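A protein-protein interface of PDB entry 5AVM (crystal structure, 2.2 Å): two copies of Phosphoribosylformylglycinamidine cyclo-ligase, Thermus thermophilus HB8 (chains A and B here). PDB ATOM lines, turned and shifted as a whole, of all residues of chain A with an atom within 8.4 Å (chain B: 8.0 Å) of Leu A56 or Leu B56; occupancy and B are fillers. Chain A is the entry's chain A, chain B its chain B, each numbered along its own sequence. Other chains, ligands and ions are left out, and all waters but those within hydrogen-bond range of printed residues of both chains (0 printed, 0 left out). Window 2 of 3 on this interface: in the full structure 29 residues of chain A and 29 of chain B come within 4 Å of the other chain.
The backbone NH (N) of Leu A99 is in hydrogen-bond range of the backbone carbonyl oxygen (O) of Val A157.
The backbone NH of Val A157 sits at hydrogen-bond distance from the backbone carbonyl oxygen of Phe A100 (2.9 Å).
The backbone carbonyl oxygen (O) of Val B157 is in hydrogen-bond range of the backbone NH (N) of Leu B99 (2.6 Å).
The backbone NH of Val B157 is in hydrogen-bond range of the backbone carbonyl oxygen of Phe B100 (3.0 Å).
Among the printed residues, pairs that only touch across the chains: Phe A100 with Leu B56 (3.7 Å), Leu A56 with Leu B56 (3.7 Å), Leu A102 with Ala B58 (3.8 Å), Ala A58 with Leu B134 (3.8 Å), Val A157 with Val B157 (3.9 Å), Leu A134 with Ala B58 (3.9 Å), Phe A100 with Ala B58 (3.97 Å) and Ala A58 with Phe B100 (3.99 Å).
Pro A54 touches none of the printed residues of chain B.
Leu A56 touches just one residue of chain B: Leu B56 (3.7 Å).
Printed residues of chain B within 4 Å of Phe A100: Leu B56 and Ala B58.
Printed residues of chain B within 4 Å of Leu A134: Ala B58.
Of the printed residues of chain B, Val A157 touches Val B157.
Leu B56 touches just these residues of chain A: Leu A56 and Phe A100.
No residue of chain A comes within 4 Å of Val B57.
Of the printed residues of chain A, Phe B100 touches Ala A58.
The nearest residue of chain B that does not touch Leu A56 is Phe B100 (4.2 Å).
The nearest residue of chain A that does not touch Leu B56 is Leu A134 (4.2 Å).
Of the 20 printed residues of chain A, 6 touch a printed residue of chain B.
Hydrophobic or aromatic side chains of chain A that line the printed part of chain B: Leu A56, Ala A58, Phe A100, Leu A102, Leu A134 and Val A157.
Of the 19 printed residues of chain B, 5 touch a printed residue of chain A.
Printed residues of chain B that touch a printed residue of chain A: Leu B56, Ala B58, Phe B100, Leu B134 and Val B157.
Among the printed residues, 8 pairs touch across the chains.
Leu B56 touches its own counterpart, Leu A56.
Ala A58 touches Phe B100, and with the chains exchanged Phe A100 touches Ala B58.
Phe A100 touches Leu B56, but with the chains exchanged Leu A56 does not touch Phe B100 (4.2 Å).
Val A157 touches its own counterpart, Val B157.
Positions printed for both chains: 53, 54, 55, 56, 57, 58, 91, 94, 96, 99, 100, 134, 157, 158, 159 and 160.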
ATOM      1  N   GLU A  53      27.825  17.409  14.412  1.00  0.00           N
ATOM      2  CA  GLU A  53      28.351  18.796  14.625  1.00  0.00           C
ATOM      3  C   GLU A  53      27.257  19.860  14.625  1.00  0.00           C
ATOM      4  O   GLU A  53      26.617  20.104  13.599  1.00  0.00           O
ATOM      5  CB  GLU A  53      29.381  19.152  13.546  1.00  0.00           C
ATOM      6  CG  GLU A  53      29.555  20.661  13.335  1.00  0.00           C
ATOM      7  CD  GLU A  53      30.757  21.022  12.474  1.00  0.00           C
ATOM      8  OE1 GLU A  53      31.901  20.771  12.923  1.00  0.00           O
ATOM      9  OE2 GLU A  53      30.560  21.557  11.356  1.00  0.00           O
ATOM     10  N   PRO A  54      27.037  20.515  15.780  1.00  0.00           N
ATOM     11  CA  PRO A  54      26.020  21.567  15.923  1.00  0.00           C
ATOM     12  C   PRO A  54      26.360  22.783  15.059  1.00  0.00           C
ATOM     13  O   PRO A  54      27.525  23.147  14.929  1.00  0.00           O
ATOM     14  CB  PRO A  54      26.073  21.901  17.415  1.00  0.00           C
ATOM     15  CG  PRO A  54      26.527  20.621  18.039  1.00  0.00           C
ATOM     16  CD  PRO A  54      27.617  20.178  17.093  1.00  0.00           C
ATOM     17  N   VAL A  55      25.348  23.418  14.481  1.00  0.00           N
ATOM     18  CA  VAL A  55      25.591  24.585  13.645  1.00  0.00           C
ATOM     19  C   VAL A  55      25.435  25.879  14.436  1.00  0.00           C
ATOM     20  O   VAL A  55      25.758  26.964  13.934  1.00  0.00           O
ATOM     21  CB  VAL A  55      24.628  24.610  12.439  1.00  0.00           C
ATOM     22  CG1 VAL A  55      24.742  23.293  11.670  1.00  0.00           C
ATOM     23  CG2 VAL A  55      23.199  24.858  12.905  1.00  0.00           C
ATOM     24  N   LEU A  56      24.949  25.747  15.675  1.00  0.00           N
ATOM     25  CA  LEU A  56      24.726  26.877  16.578  1.00  0.00           C
ATOM     26  C   LEU A  56      25.712  26.928  17.735  1.00  0.00           C
ATOM     27  O   LEU A  56      26.382  25.946  18.057  1.00  0.00           O
ATOM     28  CB  LEU A  56      23.316  26.822  17.168  1.00  0.00           C
ATOM     29  CG  LEU A  56      22.121  26.790  16.221  1.00  0.00           C
ATOM     30  CD1 LEU A  56      20.864  26.800  17.058  1.00  0.00           C
ATOM     31  CD2 LEU A  56      22.142  27.980  15.275  1.00  0.00           C
ATOM     32  N   VAL A  57      25.786  28.086  18.373  1.00  0.00           N
ATOM     33  CA  VAL A  57      26.672  28.259  19.507  1.00  0.00           C
ATOM     34  C   VAL A  57      25.837  28.527  20.754  1.00  0.00           C
ATOM     35  O   VAL A  57      24.721  29.028  20.667  1.00  0.00           O
ATOM     36  CB  VAL A  57      27.679  29.396  19.246  1.00  0.00           C
ATOM     37  CG1 VAL A  57      28.285  29.865  20.534  1.00  0.00           C
ATOM     38  CG2 VAL A  57      28.789  28.882  18.340  1.00  0.00           C
ATOM     39  N   ALA A  58      26.370  28.169  21.915  1.00  0.00           N
ATOM     40  CA  ALA A  58      25.640  28.351  23.154  1.00  0.00           C
ATOM     41  C   ALA A  58      26.583  28.489  24.327  1.00  0.00           C
ATOM     42  O   ALA A  58      27.743  28.099  24.265  1.00  0.00           O
ATOM     43  CB  ALA A  58      24.700  27.157  23.380  1.00  0.00           C
ATOM     44  N   THR A  59      26.077  29.048  25.412  1.00  0.00           N
ATOM     45  CA  THR A  59      26.891  29.207  26.590  1.00  0.00           C
ATOM     46  C   THR A  59      25.998  29.298  27.805  1.00  0.00           C
ATOM     47  O   THR A  59      24.922  29.883  27.742  1.00  0.00           O
ATOM     48  CB  THR A  59      27.760  30.489  26.499  1.00  0.00           C
ATOM     49  OG1 THR A  59      28.715  30.492  27.570  1.00  0.00           O
ATOM     50  CG2 THR A  59      26.887  31.753  26.592  1.00  0.00           C
ATOM     51  N   LEU A  91      29.214  35.331  23.941  1.00  0.00           N
ATOM     52  CA  LEU A  91      28.986  34.865  22.574  1.00  0.00           C
ATOM     53  C   LEU A  91      29.472  35.845  21.517  1.00  0.00           C
ATOM     54  O   LEU A  91      29.900  35.431  20.447  1.00  0.00           O
ATOM     55  CB  LEU A  91      27.507  34.571  22.337  1.00  0.00           C
ATOM     56  CG  LEU A  91      26.873  33.455  23.162  1.00  0.00           C
ATOM     57  CD1 LEU A  91      25.618  32.994  22.448  1.00  0.00           C
ATOM     58  CD2 LEU A  91      27.842  32.296  23.328  1.00  0.00           C
ATOM     59  N   GLN A  94      32.917  35.524  20.257  1.00  0.00           N
ATOM     60  CA  GLN A  94      33.123  34.438  19.292  1.00  0.00           C
ATOM     61  C   GLN A  94      32.519  34.833  17.947  1.00  0.00           C
ATOM     62  O   GLN A  94      32.658  34.106  16.962  1.00  0.00           O
ATOM     63  CB  GLN A  94      32.442  33.158  19.776  1.00  0.00           C
ATOM     64  CG  GLN A  94      32.666  32.864  21.252  1.00  0.00           C
ATOM     65  CD  GLN A  94      31.939  31.622  21.714  1.00  0.00           C
ATOM     66  OE1 GLN A  94      31.860  31.347  22.912  1.00  0.00           O
ATOM     67  NE2 GLN A  94      31.405  30.859  20.766  1.00  0.00           N
ATOM     68  N   ALA A  96      29.167  35.535  17.647  1.00  0.00           N
ATOM     69  CA  ALA A  96      27.802  35.022  17.587  1.00  0.00           C
ATOM     70  C   ALA A  96      26.685  36.023  17.872  1.00  0.00           C
ATOM     71  O   ALA A  96      26.749  36.803  18.825  1.00  0.00           O
ATOM     72  CB  ALA A  96      27.660  33.812  18.525  1.00  0.00           C
ATOM     73  N   GLU A  97      25.660  35.988  17.025  1.00  0.00           N
ATOM     74  CA  GLU A  97      24.491  36.845  17.188  1.00  0.00           C
ATOM     75  C   GLU A  97      23.563  36.058  18.121  1.00  0.00           C
ATOM     76  O   GLU A  97      23.299  34.874  17.885  1.00  0.00           O
ATOM     77  CB  GLU A  97      23.793  37.089  15.837  1.00  0.00           C
ATOM     78  CG  GLU A  97      22.947  38.381  15.814  1.00  0.00           C
ATOM     79  CD  GLU A  97      21.458  38.140  15.610  1.00  0.00           C
ATOM     80  OE1 GLU A  97      21.055  37.879  14.461  1.00  0.00           O
ATOM     81  OE2 GLU A  97      20.687  38.212  16.591  1.00  0.00           O
ATOM     82  N   LEU A  99      20.350  34.467  19.905  1.00  0.00           N
ATOM     83  CA  LEU A  99      19.067  33.972  19.399  1.00  0.00           C
ATOM     84  C   LEU A  99      17.990  33.901  20.495  1.00  0.00           C
ATOM     85  O   LEU A  99      16.958  34.562  20.389  1.00  0.00           O
ATOM     86  CB  LEU A  99      19.259  32.604  18.740  1.00  0.00           C
ATOM     87  CG  LEU A  99      20.112  32.626  17.461  1.00  0.00           C
ATOM     88  CD1 LEU A  99      20.279  31.217  16.961  1.00  0.00           C
ATOM     89  CD2 LEU A  99      19.472  33.506  16.388  1.00  0.00           C
ATOM     90  N   PHE A 100      18.219  33.113  21.545  1.00  0.00           N
ATOM     91  CA  PHE A 100      17.241  33.019  22.630  1.00  0.00           C
ATOM     92  C   PHE A 100      17.865  32.679  23.980  1.00  0.00           C
ATOM     93  O   PHE A 100      18.974  32.139  24.046  1.00  0.00           O
ATOM     94  CB  PHE A 100      16.112  32.029  22.269  1.00  0.00           C
ATOM     95  CG  PHE A 100      16.576  30.627  21.947  1.00  0.00           C
ATOM     96  CD1 PHE A 100      16.877  29.724  22.960  1.00  0.00           C
ATOM     97  CD2 PHE A 100      16.640  30.190  20.625  1.00  0.00           C
ATOM     98  CE1 PHE A 100      17.230  28.399  22.660  1.00  0.00           C
ATOM     99  CE2 PHE A 100      16.990  28.870  20.316  1.00  0.00           C
ATOM    100  CZ  PHE A 100      17.284  27.974  21.334  1.00  0.00           C
ATOM    101  N   LEU A 102      17.305  31.232  28.237  1.00  0.00           N
ATOM    102  CA  LEU A 102      16.574  30.395  29.184  1.00  0.00           C
ATOM    103  C   LEU A 102      17.215  30.619  30.536  1.00  0.00           C
ATOM    104  O   LEU A 102      18.439  30.664  30.644  1.00  0.00           O
ATOM    105  CB  LEU A 102      16.677  28.908  28.828  1.00  0.00           C
ATOM    106  CG  LEU A 102      15.819  28.396  27.675  1.00  0.00           C
ATOM    107  CD1 LEU A 102      16.613  28.372  26.395  1.00  0.00           C
ATOM    108  CD2 LEU A 102      15.350  27.007  28.002  1.00  0.00           C
ATOM    109  N   LEU A 134      12.917  32.266  26.019  1.00  0.00           N
ATOM    110  CA  LEU A 134      12.211  31.044  25.683  1.00  0.00           C
ATOM    111  C   LEU A 134      11.641  30.286  26.875  1.00  0.00           C
ATOM    112  O   LEU A 134      10.447  30.395  27.174  1.00  0.00           O
ATOM    113  CB  LEU A 134      13.134  30.131  24.876  1.00  0.00           C
ATOM    114  CG  LEU A 134      12.445  29.328  23.783  1.00  0.00           C
ATOM    115  CD1 LEU A 134      11.873  30.269  22.747  1.00  0.00           C
ATOM    116  CD2 LEU A 134      13.442  28.394  23.154  1.00  0.00           C
ATOM    117  N   LEU A 156      22.288  31.038  27.000  1.00  0.00           N
ATOM    118  CA  LEU A 156      22.009  31.857  25.831  1.00  0.00           C
ATOM    119  C   LEU A 156      22.485  31.064  24.616  1.00  0.00           C
ATOM    120  O   LEU A 156      23.574  30.476  24.632  1.00  0.00           O
ATOM    121  CB  LEU A 156      22.760  33.198  25.889  1.00  0.00           C
ATOM    122  CG  LEU A 156      22.637  34.065  24.622  1.00  0.00           C
ATOM    123  CD1 LEU A 156      21.221  34.601  24.487  1.00  0.00           C
ATOM    124  CD2 LEU A 156      23.619  35.218  24.685  1.00  0.00           C
ATOM    125  N   VAL A 157      21.655  31.026  23.581  1.00  0.00           N
ATOM    126  CA  VAL A 157      22.005  30.329  22.360  1.00  0.00           C
ATOM    127  C   VAL A 157      22.228  31.400  21.295  1.00  0.00           C
ATOM    128  O   VAL A 157      21.557  32.434  21.296  1.00  0.00           O
ATOM    129  CB  VAL A 157      20.876  29.362  21.931  1.00  0.00           C
ATOM    130  CG1 VAL A 157      21.176  28.764  20.549  1.00  0.00           C
ATOM    131  CG2 VAL A 157      20.733  28.249  22.973  1.00  0.00           C
ATOM    132  N   GLY A 158      23.196  31.161  20.414  1.00  0.00           N
ATOM    133  CA  GLY A 158      23.497  32.114  19.363  1.00  0.00           C
ATOM    134  C   GLY A 158      23.990  31.400  18.127  1.00  0.00           C
ATOM    135  O   GLY A 158      24.088  30.165  18.110  1.00  0.00           O
ATOM    136  N   VAL A 159      24.314  32.173  17.091  1.00  0.00           N
ATOM    137  CA  VAL A 159      24.793  31.608  15.832  1.00  0.00           C
ATOM    138  C   VAL A 159      25.869  32.495  15.196  1.00  0.00           C
ATOM    139  O   VAL A 159      25.781  33.722  15.236  1.00  0.00           O
ATOM    140  CB  VAL A 159      23.607  31.421  14.849  1.00  0.00           C
ATOM    141  CG1 VAL A 159      22.999  32.776  14.503  1.00  0.00           C
ATOM    142  CG2 VAL A 159      24.062  30.663  13.609  1.00  0.00           C
ATOM    143  N   VAL A 160      26.889  31.866  14.616  1.00  0.00           N
ATOM    144  CA  VAL A 160      27.982  32.596  13.976  1.00  0.00           C
ATOM    145  C   VAL A 160      27.900  32.550  12.447  1.00  0.00           C
ATOM    146  O   VAL A 160      27.823  31.478  11.850  1.00  0.00           O
ATOM    147  CB  VAL A 160      29.351  32.032  14.410  1.00  0.00           C
ATOM    148  CG1 VAL A 160      30.475  32.760  13.686  1.00  0.00           C
ATOM    149  CG2 VAL A 160      29.510  32.164  15.910  1.00  0.00           C
ATOM    150  N   GLU B  53       9.495  23.065   8.356  1.00  0.00           N
ATOM    151  CA  GLU B  53       9.022  24.081   9.299  1.00  0.00           C
ATOM    152  C   GLU B  53       9.674  23.826  10.654  1.00  0.00           C
ATOM    153  O   GLU B  53       8.988  23.650  11.655  1.00  0.00           O
ATOM    154  CB  GLU B  53       7.489  24.073   9.443  1.00  0.00           C
ATOM    155  CG  GLU B  53       6.764  22.796   8.999  1.00  0.00           C
ATOM    156  CD  GLU B  53       5.236  22.918   9.086  1.00  0.00           C
ATOM    157  OE1 GLU B  53       4.691  22.881  10.205  1.00  0.00           O
ATOM    158  OE2 GLU B  53       4.576  23.061   8.035  1.00  0.00           O
ATOM    159  N   PRO B  54      11.021  23.803  10.698  1.00  0.00           N
ATOM    160  CA  PRO B  54      11.754  23.564  11.941  1.00  0.00           C
ATOM    161  C   PRO B  54      11.660  24.719  12.929  1.00  0.00           C
ATOM    162  O   PRO B  54      11.807  25.885  12.558  1.00  0.00           O
ATOM    163  CB  PRO B  54      13.180  23.321  11.454  1.00  0.00           C
ATOM    164  CG  PRO B  54      13.273  24.228  10.271  1.00  0.00           C
ATOM    165  CD  PRO B  54      11.960  23.991   9.571  1.00  0.00           C
ATOM    166  N   VAL B  55      11.405  24.383  14.190  1.00  0.00           N
ATOM    167  CA  VAL B  55      11.294  25.381  15.243  1.00  0.00           C
ATOM    168  C   VAL B  55      12.268  25.029  16.350  1.00  0.00           C
ATOM    169  O   VAL B  55      12.262  23.906  16.852  1.00  0.00           O
ATOM    170  CB  VAL B  55       9.869  25.411  15.854  1.00  0.00           C
ATOM    171  CG1 VAL B  55       9.800  26.440  16.974  1.00  0.00           C
ATOM    172  CG2 VAL B  55       8.834  25.709  14.763  1.00  0.00           C
ATOM    173  N   LEU B  56      13.116  25.978  16.724  1.00  0.00           N
ATOM    174  CA  LEU B  56      14.051  25.730  17.798  1.00  0.00           C
ATOM    175  C   LEU B  56      13.306  25.798  19.123  1.00  0.00           C
ATOM    176  O   LEU B  56      12.532  26.725  19.379  1.00  0.00           O
ATOM    177  CB  LEU B  56      15.182  26.758  17.792  1.00  0.00           C
ATOM    178  CG  LEU B  56      16.162  26.719  16.615  1.00  0.00           C
ATOM    179  CD1 LEU B  56      17.255  27.748  16.838  1.00  0.00           C
ATOM    180  CD2 LEU B  56      16.767  25.333  16.480  1.00  0.00           C
ATOM    181  N   VAL B  57      13.528  24.785  19.949  1.00  0.00           N
ATOM    182  CA  VAL B  57      12.923  24.705  21.265  1.00  0.00           C
ATOM    183  C   VAL B  57      14.029  24.364  22.252  1.00  0.00           C
ATOM    184  O   VAL B  57      15.145  24.023  21.864  1.00  0.00           O
ATOM    185  CB  VAL B  57      11.836  23.606  21.330  1.00  0.00           C
ATOM    186  CG1 VAL B  57      10.658  23.988  20.457  1.00  0.00           C
ATOM    187  CG2 VAL B  57      12.406  22.278  20.883  1.00  0.00           C
ATOM    188  N   ALA B  58      13.729  24.477  23.534  1.00  0.00           N
ATOM    189  CA  ALA B  58      14.715  24.153  24.546  1.00  0.00           C
ATOM    190  C   ALA B  58      14.059  24.123  25.912  1.00  0.00           C
ATOM    191  O   ALA B  58      12.926  24.581  26.099  1.00  0.00           O
ATOM    192  CB  ALA B  58      15.869  25.172  24.530  1.00  0.00           C
ATOM    193  N   LEU B  91      11.533  17.921  26.606  1.00  0.00           N
ATOM    194  CA  LEU B  91      11.534  18.307  25.203  1.00  0.00           C
ATOM    195  C   LEU B  91      10.603  17.381  24.418  1.00  0.00           C
ATOM    196  O   LEU B  91       9.860  17.837  23.551  1.00  0.00           O
ATOM    197  CB  LEU B  91      12.961  18.250  24.639  1.00  0.00           C
ATOM    198  CG  LEU B  91      13.502  19.537  24.000  1.00  0.00           C
ATOM    199  CD1 LEU B  91      13.577  20.653  25.028  1.00  0.00           C
ATOM    200  CD2 LEU B  91      14.876  19.277  23.426  1.00  0.00           C
ATOM    201  N   GLN B  94       7.148  18.374  24.162  1.00  0.00           N
ATOM    202  CA  GLN B  94       6.856  19.428  23.193  1.00  0.00           C
ATOM    203  C   GLN B  94       6.720  18.848  21.779  1.00  0.00           C
ATOM    204  O   GLN B  94       6.095  19.447  20.904  1.00  0.00           O
ATOM    205  CB  GLN B  94       7.978  20.476  23.208  1.00  0.00           C
ATOM    206  CG  GLN B  94       8.178  21.161  24.552  1.00  0.00           C
ATOM    207  CD  GLN B  94       9.239  22.247  24.503  1.00  0.00           C
ATOM    208  OE1 GLN B  94       9.218  23.111  23.625  1.00  0.00           O
ATOM    209  NE2 GLN B  94      10.170  22.215  25.454  1.00  0.00           N
ATOM    210  N   ALA B  96       9.661  17.526  20.303  1.00  0.00           N
ATOM    211  CA  ALA B  96      10.972  17.721  19.703  1.00  0.00           C
ATOM    212  C   ALA B  96      12.033  16.663  19.963  1.00  0.00           C
ATOM    213  O   ALA B  96      11.913  15.848  20.877  1.00  0.00           O
ATOM    214  CB  ALA B  96      11.512  19.088  20.117  1.00  0.00           C
ATOM    215  N   LEU B  99      19.100  18.377  20.075  1.00  0.00           N
ATOM    216  CA  LEU B  99      20.151  18.867  19.173  1.00  0.00           C
ATOM    217  C   LEU B  99      21.514  18.942  19.887  1.00  0.00           C
ATOM    218  O   LEU B  99      22.551  18.672  19.283  1.00  0.00           O
ATOM    219  CB  LEU B  99      19.800  20.254  18.613  1.00  0.00           C
ATOM    220  CG  LEU B  99      18.833  20.359  17.429  1.00  0.00           C
ATOM    221  CD1 LEU B  99      18.577  21.835  17.110  1.00  0.00           C
ATOM    222  CD2 LEU B  99      19.417  19.646  16.218  1.00  0.00           C
ATOM    223  N   PHE B 100      21.510  19.320  21.163  1.00  0.00           N
ATOM    224  CA  PHE B 100      22.741  19.403  21.941  1.00  0.00           C
ATOM    225  C   PHE B 100      22.466  19.818  23.388  1.00  0.00           C
ATOM    226  O   PHE B 100      21.444  20.439  23.679  1.00  0.00           O
ATOM    227  CB  PHE B 100      23.742  20.363  21.273  1.00  0.00           C
ATOM    228  CG  PHE B 100      23.228  21.769  21.086  1.00  0.00           C
ATOM    229  CD1 PHE B 100      23.190  22.661  22.156  1.00  0.00           C
ATOM    230  CD2 PHE B 100      22.813  22.211  19.829  1.00  0.00           C
ATOM    231  CE1 PHE B 100      22.753  23.971  21.975  1.00  0.00           C
ATOM    232  CE2 PHE B 100      22.370  23.519  19.640  1.00  0.00           C
ATOM    233  CZ  PHE B 100      22.342  24.402  20.716  1.00  0.00           C
ATOM    234  N   LEU B 134      28.043  20.200  24.649  1.00  0.00           N
ATOM    235  CA  LEU B 134      28.761  21.470  24.539  1.00  0.00           C
ATOM    236  C   LEU B 134      29.531  21.833  25.819  1.00  0.00           C
ATOM    237  O   LEU B 134      29.306  21.260  26.886  1.00  0.00           O
ATOM    238  CB  LEU B 134      27.778  22.596  24.188  1.00  0.00           C
ATOM    239  CG  LEU B 134      27.576  22.908  22.699  1.00  0.00           C
ATOM    240  CD1 LEU B 134      27.339  21.631  21.913  1.00  0.00           C
ATOM    241  CD2 LEU B 134      26.414  23.871  22.534  1.00  0.00           C
ATOM    242  N   VAL B 157      18.783  21.765  23.903  1.00  0.00           N
ATOM    243  CA  VAL B 157      18.187  22.443  22.755  1.00  0.00           C
ATOM    244  C   VAL B 157      17.727  21.363  21.788  1.00  0.00           C
ATOM    245  O   VAL B 157      18.360  20.317  21.663  1.00  0.00           O
ATOM    246  CB  VAL B 157      19.209  23.387  22.056  1.00  0.00           C
ATOM    247  CG1 VAL B 157      18.595  24.010  20.802  1.00  0.00           C
ATOM    248  CG2 VAL B 157      19.649  24.475  23.027  1.00  0.00           C
ATOM    249  N   GLY B 158      16.616  21.609  21.112  1.00  0.00           N
ATOM    250  CA  GLY B 158      16.102  20.615  20.195  1.00  0.00           C
ATOM    251  C   GLY B 158      15.424  21.247  19.011  1.00  0.00           C
ATOM    252  O   GLY B 158      15.570  22.441  18.779  1.00  0.00           O
ATOM    253  N   VAL B 159      14.678  20.453  18.258  1.00  0.00           N
ATOM    254  CA  VAL B 159      13.999  20.977  17.088  1.00  0.00           C
ATOM    255  C   VAL B 159      12.711  20.194  16.854  1.00  0.00           C
ATOM    256  O   VAL B 159      12.629  19.011  17.168  1.00  0.00           O
ATOM    257  CB  VAL B 159      14.936  20.902  15.838  1.00  0.00           C
ATOM    258  CG1 VAL B 159      15.259  19.438  15.500  1.00  0.00           C
ATOM    259  CG2 VAL B 159      14.306  21.629  14.657  1.00  0.00           C
ATOM    260  N   VAL B 160      11.700  20.867  16.320  1.00  0.00           N
ATOM    261  CA  VAL B 160      10.413  20.237  16.050  1.00  0.00           C
ATOM    262  C   VAL B 160       9.724  20.954  14.883  1.00  0.00           C
ATOM    263  O   VAL B 160       9.903  22.156  14.700  1.00  0.00           O
ATOM    264  CB  VAL B 160       9.512  20.309  17.307  1.00  0.00           C
ATOM    265  CG1 VAL B 160       9.304  21.759  17.706  1.00  0.00           C
ATOM    266  CG2 VAL B 160       8.184  19.607  17.052  1.00  0.00           C
ATOM    267  N   GLU B 161       8.967  20.219  14.075  1.00  0.00           N
ATOM    268  CA  GLU B 161       8.251  20.838  12.960  1.00  0.00           C
ATOM    269  C   GLU B 161       7.043  21.508  13.594  1.00  0.00           C
ATOM    270  O   GLU B 161       6.308  20.876  14.352  1.00  0.00           O
ATOM    271  CB  GLU B 161       7.814  19.786  11.943  1.00  0.00           C
ATOM    272  CG  GLU B 161       8.977  19.057  11.279  1.00  0.00           C
ATOM    273  CD  GLU B 161       9.720  19.915  10.269  1.00  0.00           C
ATOM    274  OE1 GLU B 161      10.969  19.993  10.350  1.00  0.00           O
ATOM    275  OE2 GLU B 161       9.054  20.500   9.390  1.00  0.00           O
ATOM    276  N   ARG B 162       6.853  22.787  13.283  1.00  0.00           N
ATOM    277  CA  ARG B 162       5.768  23.586  13.851  1.00  0.00           C
ATOM    278  C   ARG B 162       4.411  22.905  13.958  1.00  0.00           C
ATOM    279  O   ARG B 162       3.794  22.897  15.023  1.00  0.00           O
ATOM    280  CB  ARG B 162       5.617  24.886  13.065  1.00  0.00           C
ATOM    281  CG  ARG B 162       4.713  25.929  13.722  1.00  0.00           C
ATOM    282  CD  ARG B 162       3.608  26.321  12.764  1.00  0.00           C
ATOM    283  NE  ARG B 162       4.118  26.430  11.402  1.00  0.00           N
ATOM    284  CZ  ARG B 162       3.401  26.186  10.315  1.00  0.00           C
ATOM    285  NH1 ARG B 162       2.137  25.815  10.424  1.00  0.00           N
ATOM    286  NH2 ARG B 162       3.951  26.308   9.117  1.00  0.00           N
ATOM    287  N   ILE B 165       4.019  20.084  16.750  1.00  0.00           N
ATOM    288  CA  ILE B 165       4.268  20.424  18.148  1.00  0.00           C
ATOM    289  C   ILE B 165       3.103  19.901  18.983  1.00  0.00           C
ATOM    290  O   ILE B 165       1.935  20.138  18.657  1.00  0.00           O
ATOM    291  CB  ILE B 165       4.372  21.970  18.363  1.00  0.00           C
ATOM    292  CG1 ILE B 165       5.629  22.514  17.688  1.00  0.00           C
ATOM    293  CG2 ILE B 165       4.409  22.299  19.848  1.00  0.00           C
ATOM    294  CD1 ILE B 165       5.747  24.011  17.762  1.00  0.00           C
